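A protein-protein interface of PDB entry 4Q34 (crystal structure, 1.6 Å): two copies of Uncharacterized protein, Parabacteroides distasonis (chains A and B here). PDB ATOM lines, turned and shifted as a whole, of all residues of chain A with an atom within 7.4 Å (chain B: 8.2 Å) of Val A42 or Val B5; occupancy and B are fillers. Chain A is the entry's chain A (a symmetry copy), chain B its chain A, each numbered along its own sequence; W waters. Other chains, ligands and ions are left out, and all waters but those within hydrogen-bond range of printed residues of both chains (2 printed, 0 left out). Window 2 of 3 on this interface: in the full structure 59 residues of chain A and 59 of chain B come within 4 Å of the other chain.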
ATOM      1  N   VAL A   5      13.827  -1.424   2.843  1.00  0.00           N
ATOM      2  CA  VAL A   5      13.683  -2.563   1.904  1.00  0.00           C
ATOM      3  C   VAL A   5      12.256  -2.711   1.390  1.00  0.00           C
ATOM      4  O   VAL A   5      11.288  -2.750   2.171  1.00  0.00           O
ATOM      5  CB  VAL A   5      14.148  -3.889   2.544  1.00  0.00           C
ATOM      6  CG1 VAL A   5      13.885  -5.097   1.638  1.00  0.00           C
ATOM      7  CG2 VAL A   5      15.627  -3.804   2.890  1.00  0.00           C
ATOM      8  N   LEU A   6      12.130  -2.817   0.068  1.00  0.00           N
ATOM      9  CA  LEU A   6      10.837  -2.996  -0.557  1.00  0.00           C
ATOM     10  C   LEU A   6      10.628  -4.508  -0.638  1.00  0.00           C
ATOM     11  O   LEU A   6      11.500  -5.208  -1.152  1.00  0.00           O
ATOM     12  CB  LEU A   6      10.821  -2.365  -1.933  1.00  0.00           C
ATOM     13  CG  LEU A   6      11.025  -0.865  -1.984  1.00  0.00           C
ATOM     14  CD1 LEU A   6      11.436  -0.445  -3.390  1.00  0.00           C
ATOM     15  CD2 LEU A   6       9.728  -0.181  -1.574  1.00  0.00           C
ATOM     16  N   MET A   7       9.537  -4.975  -0.037  1.00  0.00           N
ATOM     17  CA  MET A   7       9.234  -6.409   0.047  1.00  0.00           C
ATOM     18  C   MET A   7       8.266  -6.690  -1.081  1.00  0.00           C
ATOM     19  O   MET A   7       7.052  -6.464  -0.977  1.00  0.00           O
ATOM     20  CB  MET A   7       8.727  -6.799   1.444  1.00  0.00           C
ATOM     21  CG  MET A   7       9.740  -6.418   2.524  1.00  0.00           C
ATOM     22  SD  MET A   7       9.104  -6.966   4.305  1.00  0.00           S
ATOM     23  CE  MET A   7       8.636  -8.847   3.927  1.00  0.00           C
ATOM     24  N   VAL A   8       8.799  -7.185  -2.180  1.00  0.00           N
ATOM     25  CA  VAL A   8       7.999  -7.414  -3.399  1.00  0.00           C
ATOM     26  C   VAL A   8       7.506  -8.864  -3.477  1.00  0.00           C
ATOM     27  O   VAL A   8       8.256  -9.771  -3.677  1.00  0.00           O
ATOM     28  CB  VAL A   8       8.804  -7.022  -4.656  1.00  0.00           C
ATOM     29  CG1 VAL A   8       7.973  -7.267  -5.912  1.00  0.00           C
ATOM     30  CG2 VAL A   8       9.255  -5.563  -4.569  1.00  0.00           C
ATOM     31  N   ASP A   9       6.211  -9.045  -3.319  1.00  0.00           N
ATOM     32  CA  ASP A   9       5.565 -10.354  -3.365  1.00  0.00           C
ATOM     33  C   ASP A   9       5.491 -10.885  -4.819  1.00  0.00           C
ATOM     34  O   ASP A   9       5.665 -12.070  -5.069  1.00  0.00           O
ATOM     35  CB  ASP A   9       4.140 -10.169  -2.818  1.00  0.00           C
ATOM     36  CG  ASP A   9       3.519 -11.424  -2.326  1.00  0.00           C
ATOM     37  OD1 ASP A   9       4.227 -12.440  -2.139  1.00  0.00           O
ATOM     38  OD2 ASP A   9       2.296 -11.340  -2.106  1.00  0.00           O
ATOM     39  N   GLU A  10       5.309  -9.965  -5.756  1.00  0.00           N
ATOM     40  CA  GLU A  10       5.119 -10.308  -7.158  1.00  0.00           C
ATOM     41  C   GLU A  10       5.547  -9.094  -7.969  1.00  0.00           C
ATOM     42  O   GLU A  10       5.288  -7.950  -7.593  1.00  0.00           O
ATOM     43  CB  GLU A  10       3.639 -10.658  -7.452  1.00  0.00           C
ATOM     44  CG  GLU A  10       3.328 -11.272  -8.814  1.00  0.00           C
ATOM     45  CD  GLU A  10       1.819 -11.582  -9.015  1.00  0.00           C
ATOM     46  OE1 GLU A  10       1.134 -11.995  -8.035  1.00  0.00           O
ATOM     47  OE2 GLU A  10       1.327 -11.426 -10.161  1.00  0.00           O
ATOM     48  N   LYS A  40       3.605  -5.876  -6.721  1.00  0.00           N
ATOM     49  CA  LYS A  40       2.671  -6.104  -5.634  1.00  0.00           C
ATOM     50  C   LYS A  40       3.493  -6.297  -4.364  1.00  0.00           C
ATOM     51  O   LYS A  40       4.341  -7.196  -4.305  1.00  0.00           O
ATOM     52  CB  LYS A  40       1.860  -7.392  -5.862  1.00  0.00           C
ATOM     53  CG  LYS A  40       1.149  -7.425  -7.192  1.00  0.00           C
ATOM     54  CD  LYS A  40      -0.014  -8.411  -7.185  1.00  0.00           C
ATOM     55  CE  LYS A  40      -0.666  -8.477  -8.564  1.00  0.00           C
ATOM     56  NZ  LYS A  40      -1.552  -9.670  -8.719  1.00  0.00           N
ATOM     57  N   PRO A  41       3.301  -5.436  -3.373  1.00  0.00           N
ATOM     58  CA  PRO A  41       3.981  -5.607  -2.098  1.00  0.00           C
ATOM     59  C   PRO A  41       3.367  -6.685  -1.237  1.00  0.00           C
ATOM     60  O   PRO A  41       2.188  -7.048  -1.402  1.00  0.00           O
ATOM     61  CB  PRO A  41       3.842  -4.254  -1.439  1.00  0.00           C
ATOM     62  CG  PRO A  41       2.544  -3.697  -1.965  1.00  0.00           C
ATOM     63  CD  PRO A  41       2.353  -4.309  -3.353  1.00  0.00           C
ATOM     64  N   VAL A  42       4.177  -7.214  -0.337  1.00  0.00           N
ATOM     65  CA  VAL A  42       3.660  -8.026   0.751  1.00  0.00           C
ATOM     66  C   VAL A  42       2.632  -7.214   1.520  1.00  0.00           C
ATOM     67  O   VAL A  42       2.846  -6.032   1.817  1.00  0.00           O
ATOM     68  CB  VAL A  42       4.788  -8.490   1.687  1.00  0.00           C
ATOM     69  CG1 VAL A  42       4.243  -9.191   2.951  1.00  0.00           C
ATOM     70  CG2 VAL A  42       5.712  -9.452   0.954  1.00  0.00           C
ATOM     71  N   GLY A  43       1.497  -7.847   1.776  1.00  0.00           N
ATOM     72  CA  GLY A  43       0.424  -7.224   2.530  1.00  0.00           C
ATOM     73  C   GLY A  43      -0.282  -6.087   1.791  1.00  0.00           C
ATOM     74  O   GLY A  43      -0.695  -5.113   2.417  1.00  0.00           O
ATOM     75  N   ALA A  44      -0.408  -6.221   0.466  1.00  0.00           N
ATOM     76  CA  ALA A  44      -0.974  -5.183  -0.382  1.00  0.00           C
ATOM     77  C   ALA A  44      -2.390  -4.772   0.025  1.00  0.00           C
ATOM     78  O   ALA A  44      -3.220  -5.604   0.425  1.00  0.00           O
ATOM     79  CB  ALA A  44      -0.972  -5.614  -1.827  1.00  0.00           C
ATOM     80  N   ARG A  45      -2.648  -3.481  -0.104  1.00  0.00           N
ATOM     81  CA  ARG A  45      -3.939  -2.888   0.075  1.00  0.00           C
ATOM     82  C   ARG A  45      -4.902  -3.338  -1.033  1.00  0.00           C
ATOM     83  O   ARG A  45      -4.493  -3.856  -2.064  1.00  0.00           O
ATOM     84  CB  ARG A  45      -3.830  -1.355   0.092  1.00  0.00           C
ATOM     85  CG  ARG A  45      -2.946  -0.785   1.202  1.00  0.00           C
ATOM     86  CD  ARG A  45      -2.713   0.700   1.084  1.00  0.00           C
ATOM     87  NE  ARG A  45      -1.672   1.131   2.008  1.00  0.00           N
ATOM     88  CZ  ARG A  45      -1.822   1.251   3.319  1.00  0.00           C
ATOM     89  NH1 ARG A  45      -3.016   1.121   3.863  1.00  0.00           N
ATOM     90  NH2 ARG A  45      -0.786   1.602   4.072  1.00  0.00           N
ATOM     91  N   LEU A  77       4.736   1.811  -3.380  1.00  0.00           N
ATOM     92  CA  LEU A  77       5.016   0.402  -3.126  1.00  0.00           C
ATOM     93  C   LEU A  77       5.407   0.214  -1.666  1.00  0.00           C
ATOM     94  O   LEU A  77       4.937  -0.726  -1.010  1.00  0.00           O
ATOM     95  CB  LEU A  77       6.157  -0.072  -4.038  1.00  0.00           C
ATOM     96  CG  LEU A  77       6.515  -1.550  -3.917  1.00  0.00           C
ATOM     97  CD1 LEU A  77       5.316  -2.411  -4.268  1.00  0.00           C
ATOM     98  CD2 LEU A  77       7.711  -1.847  -4.814  1.00  0.00           C
ATOM     99  N   ARG A  78       6.226   1.117  -1.149  1.00  0.00           N
ATOM    100  CA  ARG A  78       6.645   1.066   0.265  1.00  0.00           C
ATOM    101  C   ARG A  78       5.461   1.222   1.219  1.00  0.00           C
ATOM    102  O   ARG A  78       5.437   0.640   2.322  1.00  0.00           O
ATOM    103  CB  ARG A  78       7.726   2.114   0.537  1.00  0.00           C
ATOM    104  CG  ARG A  78       8.309   1.969   1.922  1.00  0.00           C
ATOM    105  CD  ARG A  78       9.513   2.886   2.101  1.00  0.00           C
ATOM    106  NE  ARG A  78      10.639   2.421   1.293  1.00  0.00           N
ATOM    107  CZ  ARG A  78      11.109   3.047   0.221  1.00  0.00           C
ATOM    108  NH1 ARG A  78      10.616   4.225  -0.136  1.00  0.00           N
ATOM    109  NH2 ARG A  78      12.122   2.506  -0.446  1.00  0.00           N
ATOM    110  N   ARG A  79       4.472   1.972   0.796  1.00  0.00           N
ATOM    111  CA  ARG A  79       3.234   2.197   1.537  1.00  0.00           C
ATOM    112  C   ARG A  79       2.178   1.111   1.341  1.00  0.00           C
ATOM    113  O   ARG A  79       1.016   1.278   1.712  1.00  0.00           O
ATOM    114  CB  ARG A  79       2.693   3.570   1.155  1.00  0.00           C
ATOM    115  CG  ARG A  79       3.620   4.693   1.585  1.00  0.00           C
ATOM    116  CD  ARG A  79       3.175   6.086   1.177  1.00  0.00           C
ATOM    117  NE  ARG A  79       4.231   7.042   1.552  1.00  0.00           N
ATOM    118  CZ  ARG A  79       4.060   8.335   1.792  1.00  0.00           C
ATOM    119  NH1 ARG A  79       2.859   8.911   1.682  1.00  0.00           N
ATOM    120  NH2 ARG A  79       5.126   9.055   2.140  1.00  0.00           N
ATOM    121  N   ARG A  80       2.610   0.031   0.706  1.00  0.00           N
ATOM    122  CA  ARG A  80       1.870  -1.218   0.544  1.00  0.00           C
ATOM    123  C   ARG A  80       0.774  -1.205  -0.500  1.00  0.00           C
ATOM    124  O   ARG A  80      -0.166  -1.974  -0.396  1.00  0.00           O
ATOM    125  CB  ARG A  80       1.343  -1.733   1.883  1.00  0.00           C
ATOM    126  CG  ARG A  80       2.441  -2.017   2.892  1.00  0.00           C
ATOM    127  CD  ARG A  80       1.978  -3.006   3.976  1.00  0.00           C
ATOM    128  NE  ARG A  80       0.511  -3.101   4.029  1.00  0.00           N
ATOM    129  CZ  ARG A  80      -0.302  -2.353   4.777  1.00  0.00           C
ATOM    130  NH1 ARG A  80       0.169  -1.441   5.621  1.00  0.00           N
ATOM    131  NH2 ARG A  80      -1.606  -2.541   4.692  1.00  0.00           N
ATOM    132  N   PHE A  81       0.879  -0.308  -1.483  1.00  0.00           N
ATOM    133  CA  PHE A  81       0.003  -0.361  -2.640  1.00  0.00           C
ATOM    134  C   PHE A  81       0.660  -1.192  -3.755  1.00  0.00           C
ATOM    135  O   PHE A  81       1.868  -1.056  -4.023  1.00  0.00           O
ATOM    136  CB  PHE A  81      -0.291   1.022  -3.213  1.00  0.00           C
ATOM    137  CG  PHE A  81      -1.114   1.915  -2.326  1.00  0.00           C
ATOM    138  CD1 PHE A  81      -0.488   2.687  -1.352  1.00  0.00           C
ATOM    139  CD2 PHE A  81      -2.496   2.015  -2.478  1.00  0.00           C
ATOM    140  CE1 PHE A  81      -1.224   3.535  -0.552  1.00  0.00           C
ATOM    141  CE2 PHE A  81      -3.233   2.889  -1.698  1.00  0.00           C
ATOM    142  CZ  PHE A  81      -2.580   3.652  -0.731  1.00  0.00           C
ATOM    143  N   GLU B   3       4.240 -17.375  -3.030  1.00  0.00           N
ATOM    144  CA  GLU B   3       4.528 -16.976  -1.612  1.00  0.00           C
ATOM    145  C   GLU B   3       5.987 -16.505  -1.379  1.00  0.00           C
ATOM    146  O   GLU B   3       6.307 -16.026  -0.293  1.00  0.00           O
ATOM    147  CB  GLU B   3       4.165 -18.115  -0.645  1.00  0.00           C
ATOM    148  N   ARG B   4       6.866 -16.640  -2.378  1.00  0.00           N
ATOM    149  CA  ARG B   4       8.240 -16.128  -2.241  1.00  0.00           C
ATOM    150  C   ARG B   4       8.236 -14.597  -2.347  1.00  0.00           C
ATOM    151  O   ARG B   4       7.251 -14.001  -2.841  1.00  0.00           O
ATOM    152  CB  ARG B   4       9.189 -16.766  -3.260  1.00  0.00           C
ATOM    153  CG  ARG B   4       9.337 -18.277  -3.103  1.00  0.00           C
ATOM    154  CD  ARG B   4      10.019 -18.889  -4.312  1.00  0.00           C
ATOM    155  NE  ARG B   4       9.351 -18.499  -5.549  1.00  0.00           N
ATOM    156  CZ  ARG B   4       9.900 -18.582  -6.757  1.00  0.00           C
ATOM    157  NH1 ARG B   4      11.150 -19.033  -6.892  1.00  0.00           N
ATOM    158  NH2 ARG B   4       9.212 -18.185  -7.828  1.00  0.00           N
ATOM    159  N   VAL B   5       9.316 -13.965  -1.839  1.00  0.00           N
ATOM    160  CA  VAL B   5       9.401 -12.487  -1.751  1.00  0.00           C
ATOM    161  C   VAL B   5      10.760 -11.959  -2.192  1.00  0.00           C
ATOM    162  O   VAL B   5      11.817 -12.419  -1.722  1.00  0.00           O
ATOM    163  CB  VAL B   5       9.081 -11.984  -0.326  1.00  0.00           C
ATOM    164  CG1 VAL B   5       9.290 -10.473  -0.181  1.00  0.00           C
ATOM    165  CG2 VAL B   5       7.653 -12.355   0.043  1.00  0.00           C
ATOM    166  N   LEU B   6      10.730 -10.970  -3.084  1.00  0.00           N
ATOM    167  CA  LEU B   6      11.945 -10.349  -3.567  1.00  0.00           C
ATOM    168  C   LEU B   6      12.215  -9.184  -2.615  1.00  0.00           C
ATOM    169  O   LEU B   6      11.322  -8.366  -2.398  1.00  0.00           O
ATOM    170  CB  LEU B   6      11.763  -9.864  -4.990  1.00  0.00           C
ATOM    171  CG  LEU B   6      11.482 -10.930  -6.029  1.00  0.00           C
ATOM    172  CD1 LEU B   6      10.884 -10.291  -7.277  1.00  0.00           C
ATOM    173  CD2 LEU B   6      12.785 -11.645  -6.360  1.00  0.00           C
ATOM    174  N   MET B   7      13.392  -9.204  -1.995  1.00  0.00           N
ATOM    175  CA  MET B   7      13.772  -8.204  -0.989  1.00  0.00           C
ATOM    176  C   MET B   7      14.609  -7.181  -1.724  1.00  0.00           C
ATOM    177  O   MET B   7      15.814  -7.357  -1.952  1.00  0.00           O
ATOM    178  CB  MET B   7      14.463  -8.854   0.220  1.00  0.00           C
ATOM    179  CG  MET B   7      13.571  -9.919   0.858  1.00  0.00           C
ATOM    180  SD  MET B   7      14.444 -10.710   2.435  1.00  0.00           S
ATOM    181  CE  MET B   7      14.954  -9.062   3.396  1.00  0.00           C
ATOM    182  N   VAL B   8      13.971  -6.094  -2.110  1.00  0.00           N
ATOM    183  CA  VAL B   8      14.627  -5.053  -2.926  1.00  0.00           C
ATOM    184  C   VAL B   8      15.177  -3.922  -2.048  1.00  0.00           C
ATOM    185  O   VAL B   8      14.452  -3.162  -1.479  1.00  0.00           O
ATOM    186  CB  VAL B   8      13.658  -4.516  -4.000  1.00  0.00           C
ATOM    187  CG1 VAL B   8      14.341  -3.438  -4.835  1.00  0.00           C
ATOM    188  CG2 VAL B   8      13.151  -5.658  -4.882  1.00  0.00           C
ATOM    189  N   GLU B  70       7.901 -16.044 -14.552  1.00  0.00           N
ATOM    190  CA  GLU B  70       9.020 -15.143 -14.266  1.00  0.00           C
ATOM    191  C   GLU B  70      10.135 -15.323 -15.266  1.00  0.00           C
ATOM    192  O   GLU B  70      10.442 -16.452 -15.692  1.00  0.00           O
ATOM    193  CB  GLU B  70       9.562 -15.437 -12.865  1.00  0.00           C
ATOM    194  CG  GLU B  70       8.607 -15.037 -11.764  1.00  0.00           C
ATOM    195  CD  GLU B  70       9.351 -15.038 -10.450  1.00  0.00           C
ATOM    196  OE1 GLU B  70      10.189 -15.958 -10.262  1.00  0.00           O
ATOM    197  OE2 GLU B  70       9.182 -14.094  -9.671  1.00  0.00           O
ATOM    198  N   LEU B  77      17.418 -11.614  -9.628  1.00  0.00           N
ATOM    199  CA  LEU B  77      17.240 -10.778  -8.446  1.00  0.00           C
ATOM    200  C   LEU B  77      17.038 -11.660  -7.221  1.00  0.00           C
ATOM    201  O   LEU B  77      17.629 -11.404  -6.163  1.00  0.00           O
ATOM    202  CB  LEU B  77      16.021  -9.863  -8.638  1.00  0.00           C
ATOM    203  CG  LEU B  77      15.753  -8.890  -7.495  1.00  0.00           C
ATOM    204  CD1 LEU B  77      16.940  -7.965  -7.303  1.00  0.00           C
ATOM    205  CD2 LEU B  77      14.472  -8.117  -7.791  1.00  0.00           C
ATOM    206  N   ARG B  78      16.245 -12.710  -7.369  1.00  0.00           N
ATOM    207  CA  ARG B  78      16.004 -13.661  -6.267  1.00  0.00           C
ATOM    208  C   ARG B  78      17.286 -14.372  -5.832  1.00  0.00           C
ATOM    209  O   ARG B  78      17.471 -14.703  -4.645  1.00  0.00           O
ATOM    210  CB  ARG B  78      14.914 -14.663  -6.658  1.00  0.00           C
ATOM    211  CG  ARG B  78      14.511 -15.534  -5.494  1.00  0.00           C
ATOM    212  CD  ARG B  78      13.296 -16.381  -5.848  1.00  0.00           C
ATOM    213  NE  ARG B  78      12.103 -15.544  -5.973  1.00  0.00           N
ATOM    214  CZ  ARG B  78      11.477 -15.288  -7.115  1.00  0.00           C
ATOM    215  NH1 ARG B  78      11.865 -15.875  -8.238  1.00  0.00           N
ATOM    216  NH2 ARG B  78      10.418 -14.487  -7.100  1.00  0.00           N
HETATM  217  O   HOH W   1       4.683 -14.630  -4.176  1.00  0.00           O
HETATM  218  O   HOH W   2       8.574 -12.919  -5.233  1.00  0.00           O
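The backbone carbonyl oxygen (O) of Leu B6 sits at hydrogen-bond distance from the backbone NH (N) of Val A8, at 2.8 Å. O of Leu A6 sits at hydrogen-bond distance from N of Val B8. The backbone carbonyl oxygen (O) of Leu A6 lies close to the backbone carbonyl oxygen (O) of Leu B6 (3.4 Å). The backbone carbonyl oxygen (O) of Asp A9 sits close to the backbone carbonyl oxygen (O) of Arg B4 (3.3 Å).
OE1 of Glu B70 is in salt-bridge range of NH2 of Arg B4. The backbone carbonyl oxygen (O) of Met A7 sits at hydrogen-bond distance from the backbone NH (N) of Val A42 (3.0 Å). N of Asp A9 is in hydrogen-bond range of O of Lys A40 (2.8 Å).
Val B8 touches Val A5 (O to CA, 3.5 Å). O of Leu A6 touches C of Met B7 (3.7 Å). Met A7 touches Leu B6 (C to O, 3.7 Å). Val A8 touches Val B5. CG2 of Val B8 touches CG2 of Val A8 (3.9 Å). CG2 of Val B5 touches CG2 of Val A42, 3.6 Å away.
Of chain B, only Val B5 (3.6 Å) comes within 4 Å of Val A42. Of chain A, only Val A8 and Val A42 come within 4 Å of Val B5. Printed residues of chain A within 4 Å of Arg B4: Asp A9 (3.3 Å). Of the printed residues of chain B, Met A7 touches Leu B6. The nearest printed residue of chain A that does not touch Val B5 is Met A7 (4.02 Å). The nearest printed residue of chain A that does not touch Arg B4 is Val A8 (4.4 Å).
Of the 17 printed residues of chain A, 6 touch a printed residue of chain B. Hydrophobic or aromatic side chains of chain A that line the printed part of chain B: Val A5, Leu A6, Val A8 and Val A42. Printed residues of chain B that touch a printed residue of chain A: Arg B4, Val B5, Leu B6, Met B7 and Val B8. Hydrophobic or aromatic side chains of chain B within 4 Å of the printed part of chain A: Val B5, Leu B6 and Val B8.
Val A5 touches Val B8, and with the chains exchanged Val A8 touches Val B5. Leu B6 touches its own counterpart, Leu A6. Leu A6 touches Met B7, and with the chains exchanged Met A7 touches Leu B6. Leu A6 touches Val B8, and with the chains exchanged Val A8 touches Leu B6. 6 positions are printed for both chains.
Water W1 lies within hydrogen-bond range of the backbone carbonyl oxygen (O) of Asp A9 (2.9 Å), the backbone carbonyl oxygen (O) of Arg B4 (3.0 Å) and the backbone NH (N) of Glu B3 (3.0 Å). Water W2 lies within hydrogen-bond range of the backbone carbonyl oxygen of Arg B4 (2.9 Å), the backbone carbonyl oxygen of Asp A9 (3.0 Å) and the guanidinium group of Arg B78 (3.1 Å).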
